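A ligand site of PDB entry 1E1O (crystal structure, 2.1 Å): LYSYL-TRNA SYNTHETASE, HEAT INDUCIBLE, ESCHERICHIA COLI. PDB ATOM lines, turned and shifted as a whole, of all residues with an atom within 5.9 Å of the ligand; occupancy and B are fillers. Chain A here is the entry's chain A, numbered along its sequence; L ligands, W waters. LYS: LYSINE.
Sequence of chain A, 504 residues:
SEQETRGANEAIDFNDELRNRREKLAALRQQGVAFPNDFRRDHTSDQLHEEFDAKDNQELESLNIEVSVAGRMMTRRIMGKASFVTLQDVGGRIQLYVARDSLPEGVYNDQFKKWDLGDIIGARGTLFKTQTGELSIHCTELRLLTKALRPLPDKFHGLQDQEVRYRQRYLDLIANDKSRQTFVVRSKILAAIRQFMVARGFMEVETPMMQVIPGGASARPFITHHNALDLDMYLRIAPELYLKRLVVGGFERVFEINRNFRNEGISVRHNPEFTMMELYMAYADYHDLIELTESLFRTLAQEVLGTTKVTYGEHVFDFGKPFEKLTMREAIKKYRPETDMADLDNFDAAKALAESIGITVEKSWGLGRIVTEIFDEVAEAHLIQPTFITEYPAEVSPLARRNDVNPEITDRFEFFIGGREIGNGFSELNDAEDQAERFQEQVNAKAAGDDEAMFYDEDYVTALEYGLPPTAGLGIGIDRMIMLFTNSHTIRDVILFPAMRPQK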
ATOM      1  N   GLY A 216      -3.546  -5.895   2.096  1.00  0.00           N
ATOM      2  CA  GLY A 216      -3.839  -4.591   1.540  1.00  0.00           C
ATOM      3  C   GLY A 216      -4.816  -4.647   0.376  1.00  0.00           C
ATOM      4  O   GLY A 216      -5.198  -3.601  -0.154  1.00  0.00           O
ATOM      5  N   ALA A 217      -5.226  -5.850   0.007  1.00  0.00           N
ATOM      6  CA  ALA A 217      -6.155  -6.055  -1.103  1.00  0.00           C
ATOM      7  C   ALA A 217      -6.567  -7.523  -1.092  1.00  0.00           C
ATOM      8  O   ALA A 217      -6.081  -8.290  -0.263  1.00  0.00           O
ATOM      9  CB  ALA A 217      -5.490  -5.689  -2.420  1.00  0.00           C
ATOM     10  N   ILE A 237       0.497  -7.720  -3.327  1.00  0.00           N
ATOM     11  CA  ILE A 237      -0.716  -7.383  -4.056  1.00  0.00           C
ATOM     12  C   ILE A 237      -1.068  -5.917  -3.776  1.00  0.00           C
ATOM     13  O   ILE A 237      -1.820  -5.301  -4.527  1.00  0.00           O
ATOM     14  CB  ILE A 237      -1.904  -8.322  -3.711  1.00  0.00           C
ATOM     15  CG1 ILE A 237      -2.274  -8.225  -2.243  1.00  0.00           C
ATOM     16  CG2 ILE A 237      -1.560  -9.774  -4.076  1.00  0.00           C
ATOM     17  CD1 ILE A 237      -3.431  -9.113  -1.860  1.00  0.00           C
ATOM     18  N   ALA A 238      -0.488  -5.367  -2.707  1.00  0.00           N
ATOM     19  CA  ALA A 238      -0.663  -3.951  -2.326  1.00  0.00           C
ATOM     20  C   ALA A 238       0.284  -3.603  -1.181  1.00  0.00           C
ATOM     21  O   ALA A 238       0.613  -4.461  -0.363  1.00  0.00           O
ATOM     22  CB  ALA A 238      -2.108  -3.691  -1.905  1.00  0.00           C
ATOM     23  N   PRO A 239       0.765  -2.348  -1.117  1.00  0.00           N
ATOM     24  CA  PRO A 239       1.665  -1.913  -0.051  1.00  0.00           C
ATOM     25  C   PRO A 239       0.924  -1.340   1.159  1.00  0.00           C
ATOM     26  O   PRO A 239       1.536  -0.899   2.138  1.00  0.00           O
ATOM     27  CB  PRO A 239       2.462  -0.808  -0.736  1.00  0.00           C
ATOM     28  CG  PRO A 239       1.440  -0.161  -1.602  1.00  0.00           C
ATOM     29  CD  PRO A 239       0.756  -1.369  -2.225  1.00  0.00           C
ATOM     30  N   GLU A 240      -0.407  -1.371   1.115  1.00  0.00           N
ATOM     31  CA  GLU A 240      -1.224  -0.725   2.127  1.00  0.00           C
ATOM     32  C   GLU A 240      -0.831  -0.935   3.594  1.00  0.00           C
ATOM     33  O   GLU A 240      -0.673   0.034   4.330  1.00  0.00           O
ATOM     34  CB  GLU A 240      -2.696  -1.070   1.932  1.00  0.00           C
ATOM     35  CG  GLU A 240      -3.601  -0.533   3.057  1.00  0.00           C
ATOM     36  CD  GLU A 240      -5.085  -0.505   2.697  1.00  0.00           C
ATOM     37  OE1 GLU A 240      -5.419  -0.621   1.498  1.00  0.00           O
ATOM     38  OE2 GLU A 240      -5.915  -0.353   3.611  1.00  0.00           O
ATOM     39  N   LYS A 244       0.525   2.157   6.148  1.00  0.00           N
ATOM     40  CA  LYS A 244      -0.143   2.626   7.351  1.00  0.00           C
ATOM     41  C   LYS A 244       0.732   2.495   8.602  1.00  0.00           C
ATOM     42  O   LYS A 244       0.572   3.257   9.551  1.00  0.00           O
ATOM     43  CB  LYS A 244      -1.511   1.966   7.528  1.00  0.00           C
ATOM     44  CG  LYS A 244      -2.660   2.851   6.997  1.00  0.00           C
ATOM     45  CD  LYS A 244      -4.006   2.172   7.104  1.00  0.00           C
ATOM     46  CE  LYS A 244      -4.101   1.012   6.138  1.00  0.00           C
ATOM     47  NZ  LYS A 244      -5.417   0.342   6.273  1.00  0.00           N
ATOM     48  N   ASN A 260       2.210  -3.667  -8.295  1.00  0.00           N
ATOM     49  CA  ASN A 260       1.503  -4.648  -7.503  1.00  0.00           C
ATOM     50  C   ASN A 260       1.480  -5.845  -8.437  1.00  0.00           C
ATOM     51  O   ASN A 260       1.662  -5.697  -9.652  1.00  0.00           O
ATOM     52  CB  ASN A 260       0.072  -4.211  -7.187  1.00  0.00           C
ATOM     53  CG  ASN A 260      -0.004  -3.150  -6.105  1.00  0.00           C
ATOM     54  OD1 ASN A 260       0.906  -2.998  -5.289  1.00  0.00           O
ATOM     55  ND2 ASN A 260      -1.111  -2.420  -6.074  1.00  0.00           N
ATOM     56  N   ARG A 262      -0.748  -9.354  -9.206  1.00  0.00           N
ATOM     57  CA  ARG A 262      -1.933 -10.136  -8.919  1.00  0.00           C
ATOM     58  C   ARG A 262      -1.993 -11.273  -9.927  1.00  0.00           C
ATOM     59  O   ARG A 262      -1.892 -11.073 -11.126  1.00  0.00           O
ATOM     60  CB  ARG A 262      -3.174  -9.237  -8.895  1.00  0.00           C
ATOM     61  CG  ARG A 262      -3.070  -8.222  -7.753  1.00  0.00           C
ATOM     62  CD  ARG A 262      -4.241  -7.262  -7.594  1.00  0.00           C
ATOM     63  NE  ARG A 262      -3.885  -6.161  -6.687  1.00  0.00           N
ATOM     64  CZ  ARG A 262      -4.720  -5.193  -6.299  1.00  0.00           C
ATOM     65  NH1 ARG A 262      -5.986  -5.189  -6.695  1.00  0.00           N
ATOM     66  NH2 ARG A 262      -4.270  -4.177  -5.571  1.00  0.00           N
ATOM     67  N   MET A 276       0.527   1.215  -9.328  1.00  0.00           N
ATOM     68  CA  MET A 276      -0.491   1.793  -8.487  1.00  0.00           C
ATOM     69  C   MET A 276       0.154   2.889  -7.648  1.00  0.00           C
ATOM     70  O   MET A 276       1.324   2.773  -7.263  1.00  0.00           O
ATOM     71  CB  MET A 276      -1.052   0.705  -7.568  1.00  0.00           C
ATOM     72  CG  MET A 276      -2.149   1.154  -6.620  1.00  0.00           C
ATOM     73  SD  MET A 276      -3.785   0.832  -7.277  1.00  0.00           S
ATOM     74  CE  MET A 276      -3.867  -0.913  -7.131  1.00  0.00           C
ATOM     75  N   GLU A 278      -0.442   4.701  -4.052  1.00  0.00           N
ATOM     76  CA  GLU A 278      -1.212   4.709  -2.822  1.00  0.00           C
ATOM     77  C   GLU A 278      -0.738   5.909  -2.039  1.00  0.00           C
ATOM     78  O   GLU A 278       0.457   6.220  -2.030  1.00  0.00           O
ATOM     79  CB  GLU A 278      -1.011   3.431  -1.997  1.00  0.00           C
ATOM     80  CG  GLU A 278      -1.666   2.172  -2.565  1.00  0.00           C
ATOM     81  CD  GLU A 278      -1.992   1.157  -1.478  1.00  0.00           C
ATOM     82  OE1 GLU A 278      -2.133   1.556  -0.307  1.00  0.00           O
ATOM     83  OE2 GLU A 278      -2.143  -0.038  -1.790  1.00  0.00           O
ATOM     84  N   TYR A 280      -1.554   8.315   1.703  1.00  0.00           N
ATOM     85  CA  TYR A 280      -2.230   8.345   2.985  1.00  0.00           C
ATOM     86  C   TYR A 280      -1.998   9.692   3.615  1.00  0.00           C
ATOM     87  O   TYR A 280      -0.877  10.220   3.578  1.00  0.00           O
ATOM     88  CB  TYR A 280      -1.713   7.237   3.910  1.00  0.00           C
ATOM     89  CG  TYR A 280      -2.105   5.853   3.438  1.00  0.00           C
ATOM     90  CD1 TYR A 280      -1.394   5.215   2.422  1.00  0.00           C
ATOM     91  CD2 TYR A 280      -3.218   5.216   3.962  1.00  0.00           C
ATOM     92  CE1 TYR A 280      -1.796   3.975   1.930  1.00  0.00           C
ATOM     93  CE2 TYR A 280      -3.633   3.988   3.480  1.00  0.00           C
ATOM     94  CZ  TYR A 280      -2.919   3.372   2.462  1.00  0.00           C
ATOM     95  OH  TYR A 280      -3.388   2.182   1.947  1.00  0.00           O
ATOM     96  N   LEU A 399     -10.354  -3.306   5.755  1.00  0.00           N
ATOM     97  CA  LEU A 399      -9.394  -2.311   6.218  1.00  0.00           C
ATOM     98  C   LEU A 399      -9.995  -0.903   6.316  1.00  0.00           C
ATOM     99  O   LEU A 399      -9.275   0.061   6.616  1.00  0.00           O
ATOM    100  CB  LEU A 399      -8.189  -2.279   5.266  1.00  0.00           C
ATOM    101  CG  LEU A 399      -7.512  -3.628   5.039  1.00  0.00           C
ATOM    102  CD1 LEU A 399      -6.418  -3.523   3.982  1.00  0.00           C
ATOM    103  CD2 LEU A 399      -6.944  -4.115   6.354  1.00  0.00           C
ATOM    104  N   GLU A 414     -15.088   3.813  -4.459  1.00  0.00           N
ATOM    105  CA  GLU A 414     -14.252   3.474  -5.582  1.00  0.00           C
ATOM    106  C   GLU A 414     -14.664   4.473  -6.644  1.00  0.00           C
ATOM    107  O   GLU A 414     -15.746   5.051  -6.566  1.00  0.00           O
ATOM    108  CB  GLU A 414     -14.496   2.043  -6.033  1.00  0.00           C
ATOM    109  CG  GLU A 414     -13.943   1.036  -5.061  1.00  0.00           C
ATOM    110  CD  GLU A 414     -13.519  -0.249  -5.714  1.00  0.00           C
ATOM    111  OE1 GLU A 414     -14.095  -0.606  -6.762  1.00  0.00           O
ATOM    112  OE2 GLU A 414     -12.601  -0.914  -5.190  1.00  0.00           O
ATOM    113  N   GLU A 421     -12.640   0.585 -13.132  1.00  0.00           N
ATOM    114  CA  GLU A 421     -12.256   1.033 -11.797  1.00  0.00           C
ATOM    115  C   GLU A 421     -10.895   1.740 -11.879  1.00  0.00           C
ATOM    116  O   GLU A 421      -9.913   1.150 -12.341  1.00  0.00           O
ATOM    117  CB  GLU A 421     -12.152  -0.155 -10.842  1.00  0.00           C
ATOM    118  CG  GLU A 421     -11.859   0.235  -9.418  1.00  0.00           C
ATOM    119  CD  GLU A 421     -11.481  -0.950  -8.559  1.00  0.00           C
ATOM    120  OE1 GLU A 421     -11.984  -2.067  -8.827  1.00  0.00           O
ATOM    121  OE2 GLU A 421     -10.683  -0.761  -7.612  1.00  0.00           O
ATOM    122  N   ASN A 424      -9.569   3.490  -5.524  1.00  0.00           N
ATOM    123  CA  ASN A 424     -10.217   2.877  -4.373  1.00  0.00           C
ATOM    124  C   ASN A 424      -9.695   3.662  -3.156  1.00  0.00           C
ATOM    125  O   ASN A 424      -8.490   3.784  -2.959  1.00  0.00           O
ATOM    126  CB  ASN A 424      -9.805   1.412  -4.288  1.00  0.00           C
ATOM    127  CG  ASN A 424     -10.331   0.722  -3.055  1.00  0.00           C
ATOM    128  OD1 ASN A 424     -11.325   1.133  -2.464  1.00  0.00           O
ATOM    129  ND2 ASN A 424      -9.645  -0.342  -2.657  1.00  0.00           N
ATOM    130  N   GLY A 425     -10.611   4.231  -2.373  1.00  0.00           N
ATOM    131  CA  GLY A 425     -10.178   5.051  -1.266  1.00  0.00           C
ATOM    132  C   GLY A 425     -11.112   4.949  -0.094  1.00  0.00           C
ATOM    133  O   GLY A 425     -12.290   4.641  -0.260  1.00  0.00           O
ATOM    134  N   PHE A 426     -10.588   5.170   1.104  1.00  0.00           N
ATOM    135  CA  PHE A 426     -11.411   5.153   2.299  1.00  0.00           C
ATOM    136  C   PHE A 426     -10.794   5.806   3.529  1.00  0.00           C
ATOM    137  O   PHE A 426      -9.578   6.049   3.601  1.00  0.00           O
ATOM    138  CB  PHE A 426     -11.879   3.722   2.667  1.00  0.00           C
ATOM    139  CG  PHE A 426     -10.823   2.649   2.553  1.00  0.00           C
ATOM    140  CD1 PHE A 426      -9.967   2.355   3.614  1.00  0.00           C
ATOM    141  CD2 PHE A 426     -10.789   1.823   1.424  1.00  0.00           C
ATOM    142  CE1 PHE A 426      -9.092   1.260   3.558  1.00  0.00           C
ATOM    143  CE2 PHE A 426      -9.918   0.714   1.359  1.00  0.00           C
ATOM    144  CZ  PHE A 426      -9.075   0.437   2.443  1.00  0.00           C
ATOM    145  N   GLU A 428      -9.448   5.284   6.846  1.00  0.00           N
ATOM    146  CA  GLU A 428      -8.789   4.079   7.332  1.00  0.00           C
ATOM    147  C   GLU A 428      -9.297   3.555   8.652  1.00  0.00           C
ATOM    148  O   GLU A 428      -9.684   4.322   9.529  1.00  0.00           O
ATOM    149  CB  GLU A 428      -7.288   4.343   7.440  1.00  0.00           C
ATOM    150  CG  GLU A 428      -6.662   4.788   6.141  1.00  0.00           C
ATOM    151  CD  GLU A 428      -6.815   3.763   5.027  1.00  0.00           C
ATOM    152  OE1 GLU A 428      -6.969   2.565   5.340  1.00  0.00           O
ATOM    153  OE2 GLU A 428      -6.760   4.169   3.848  1.00  0.00           O
ATOM    154  N   GLY A 473      -6.861   7.021   3.034  1.00  0.00           N
ATOM    155  CA  GLY A 473      -5.923   6.488   2.063  1.00  0.00           C
ATOM    156  C   GLY A 473      -6.604   6.244   0.736  1.00  0.00           C
ATOM    157  O   GLY A 473      -7.797   5.937   0.686  1.00  0.00           O
ATOM    158  N   LEU A 474      -5.833   6.307  -0.340  1.00  0.00           N
ATOM    159  CA  LEU A 474      -6.380   6.182  -1.675  1.00  0.00           C
ATOM    160  C   LEU A 474      -5.396   5.453  -2.564  1.00  0.00           C
ATOM    161  O   LEU A 474      -4.196   5.710  -2.507  1.00  0.00           O
ATOM    162  CB  LEU A 474      -6.640   7.579  -2.259  1.00  0.00           C
ATOM    163  CG  LEU A 474      -7.090   7.701  -3.717  1.00  0.00           C
ATOM    164  CD1 LEU A 474      -8.471   7.094  -3.892  1.00  0.00           C
ATOM    165  CD2 LEU A 474      -7.086   9.167  -4.132  1.00  0.00           C
ATOM    166  N   GLY A 475      -5.910   4.522  -3.370  1.00  0.00           N
ATOM    167  CA  GLY A 475      -5.098   3.838  -4.365  1.00  0.00           C
ATOM    168  C   GLY A 475      -5.642   4.211  -5.736  1.00  0.00           C
ATOM    169  O   GLY A 475      -6.855   4.267  -5.930  1.00  0.00           O
ATOM    170  N   ILE A 476      -4.753   4.549  -6.666  1.00  0.00           N
ATOM    171  CA  ILE A 476      -5.150   4.926  -8.017  1.00  0.00           C
ATOM    172  C   ILE A 476      -4.362   4.081  -9.014  1.00  0.00           C
ATOM    173  O   ILE A 476      -3.127   3.994  -8.915  1.00  0.00           O
ATOM    174  CB  ILE A 476      -4.864   6.416  -8.287  1.00  0.00           C
ATOM    175  CG1 ILE A 476      -5.794   7.284  -7.432  1.00  0.00           C
ATOM    176  CG2 ILE A 476      -5.074   6.736  -9.752  1.00  0.00           C
ATOM    177  CD1 ILE A 476      -5.487   8.746  -7.526  1.00  0.00           C
HETATM  178  N   LYS L   1      -4.809  -1.089  -1.069  1.00  0.00           N
HETATM  179  CA  LYS L   1      -5.886  -0.567  -1.901  1.00  0.00           C
HETATM  180  C   LYS L   1      -5.976  -1.350  -3.213  1.00  0.00           C
HETATM  181  O   LYS L   1      -5.015  -2.075  -3.566  1.00  0.00           O
HETATM  182  CB  LYS L   1      -5.671   0.922  -2.178  1.00  0.00           C
HETATM  183  CG  LYS L   1      -5.711   1.801  -0.941  1.00  0.00           C
HETATM  184  CD  LYS L   1      -7.088   1.805  -0.300  1.00  0.00           C
HETATM  185  CE  LYS L   1      -7.145   2.713   0.924  1.00  0.00           C
HETATM  186  NZ  LYS L   1      -6.384   2.146   2.081  1.00  0.00           N
HETATM  187  OXT LYS L   1      -7.021  -1.226  -3.884  1.00  0.00           O
HETATM  188  O   HOH W   1      -2.521  -1.048  -4.196  1.00  0.00           O
HETATM  189  O   HOH W   2      -7.450  -2.463  -6.309  1.00  0.00           O
HETATM  190  O   HOH W   3      -7.240  -2.388   0.614  1.00  0.00           O
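The side-chain amide nitrogen (ND2) of Asn 424 lies within hydrogen-bond range of an oxygen (OXT) of the ligand, 3.0 Å away.
A nitrogen (N) of the ligand lies within salt-bridge range of the side-chain carboxylate (OE2) of Glu 278 (3.0 Å).
The side-chain hydroxyl of Tyr 280 lies within hydrogen-bond range of a nitrogen (NZ) of the ligand, 3.0 Å away.
The backbone carbonyl oxygen (O) of Gly 216 lies within hydrogen-bond range of a nitrogen (N) of the ligand, at 2.7 Å.
A nitrogen (N) of the ligand is in salt-bridge range of the side-chain carboxylate of Glu 240, at 2.7 Å.
A nitrogen (NZ) of the ligand lies within salt-bridge range of the side-chain carboxylate (OE2) of Glu 428, 2.7 Å away.
The guanidinium group of Arg 262 is in salt-bridge range of an oxygen (O) of the ligand, at 3.0 Å.
OE1 of Glu 428 lies within salt-bridge range of NZ of Lys 244 (2.9 Å).
The backbone carbonyl oxygen (O) of Ile 237 sits at hydrogen-bond distance from the guanidinium group (NH2) of Arg 262 (2.9 Å).
The side-chain carboxylate of Glu 240 sits close to the side-chain hydroxyl of Tyr 280.
NZ of Lys 244 is in salt-bridge range of OE2 of Glu 240 (2.8 Å).
The backbone carbonyl oxygen (O) of Asn 424 sits at hydrogen-bond distance from the backbone NH (N) of Gly 475.
The side-chain carboxylate of Glu 278 sits at hydrogen-bond distance from the side-chain hydroxyl of Tyr 280, at 2.7 Å.
The side-chain carboxylate of Glu 428 sits at hydrogen-bond distance from the backbone NH of Gly 473 (3.0 Å).
N of Phe 426 sits at hydrogen-bond distance from O of Gly 473, at 2.9 Å.
Residues that only touch the ligand: Phe 426, Gly 473, Gly 475, Ala 238, Ala 217 and Met 276.
Hydrophobic or aromatic side chains within 4 Å of the ligand: Ala 217, Ala 238, Met 276, Tyr 280 and Phe 426.
Water W2 lies within hydrogen-bond range of OXT of the ligand (2.8 Å) and NH1 of Arg 262 (3.1 Å).
Water W1 lies within hydrogen-bond range of the side-chain carboxylate (OE2) of Glu 278 (2.6 Å), the side-chain amide nitrogen (ND2) of Asn 260 (2.7 Å) and an oxygen (O) of the ligand (2.8 Å).
Water W3 lies within hydrogen-bond range of O of Gly 216 (2.5 Å), OE1 of Glu 240 (2.7 Å) and N of the ligand (3.2 Å).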
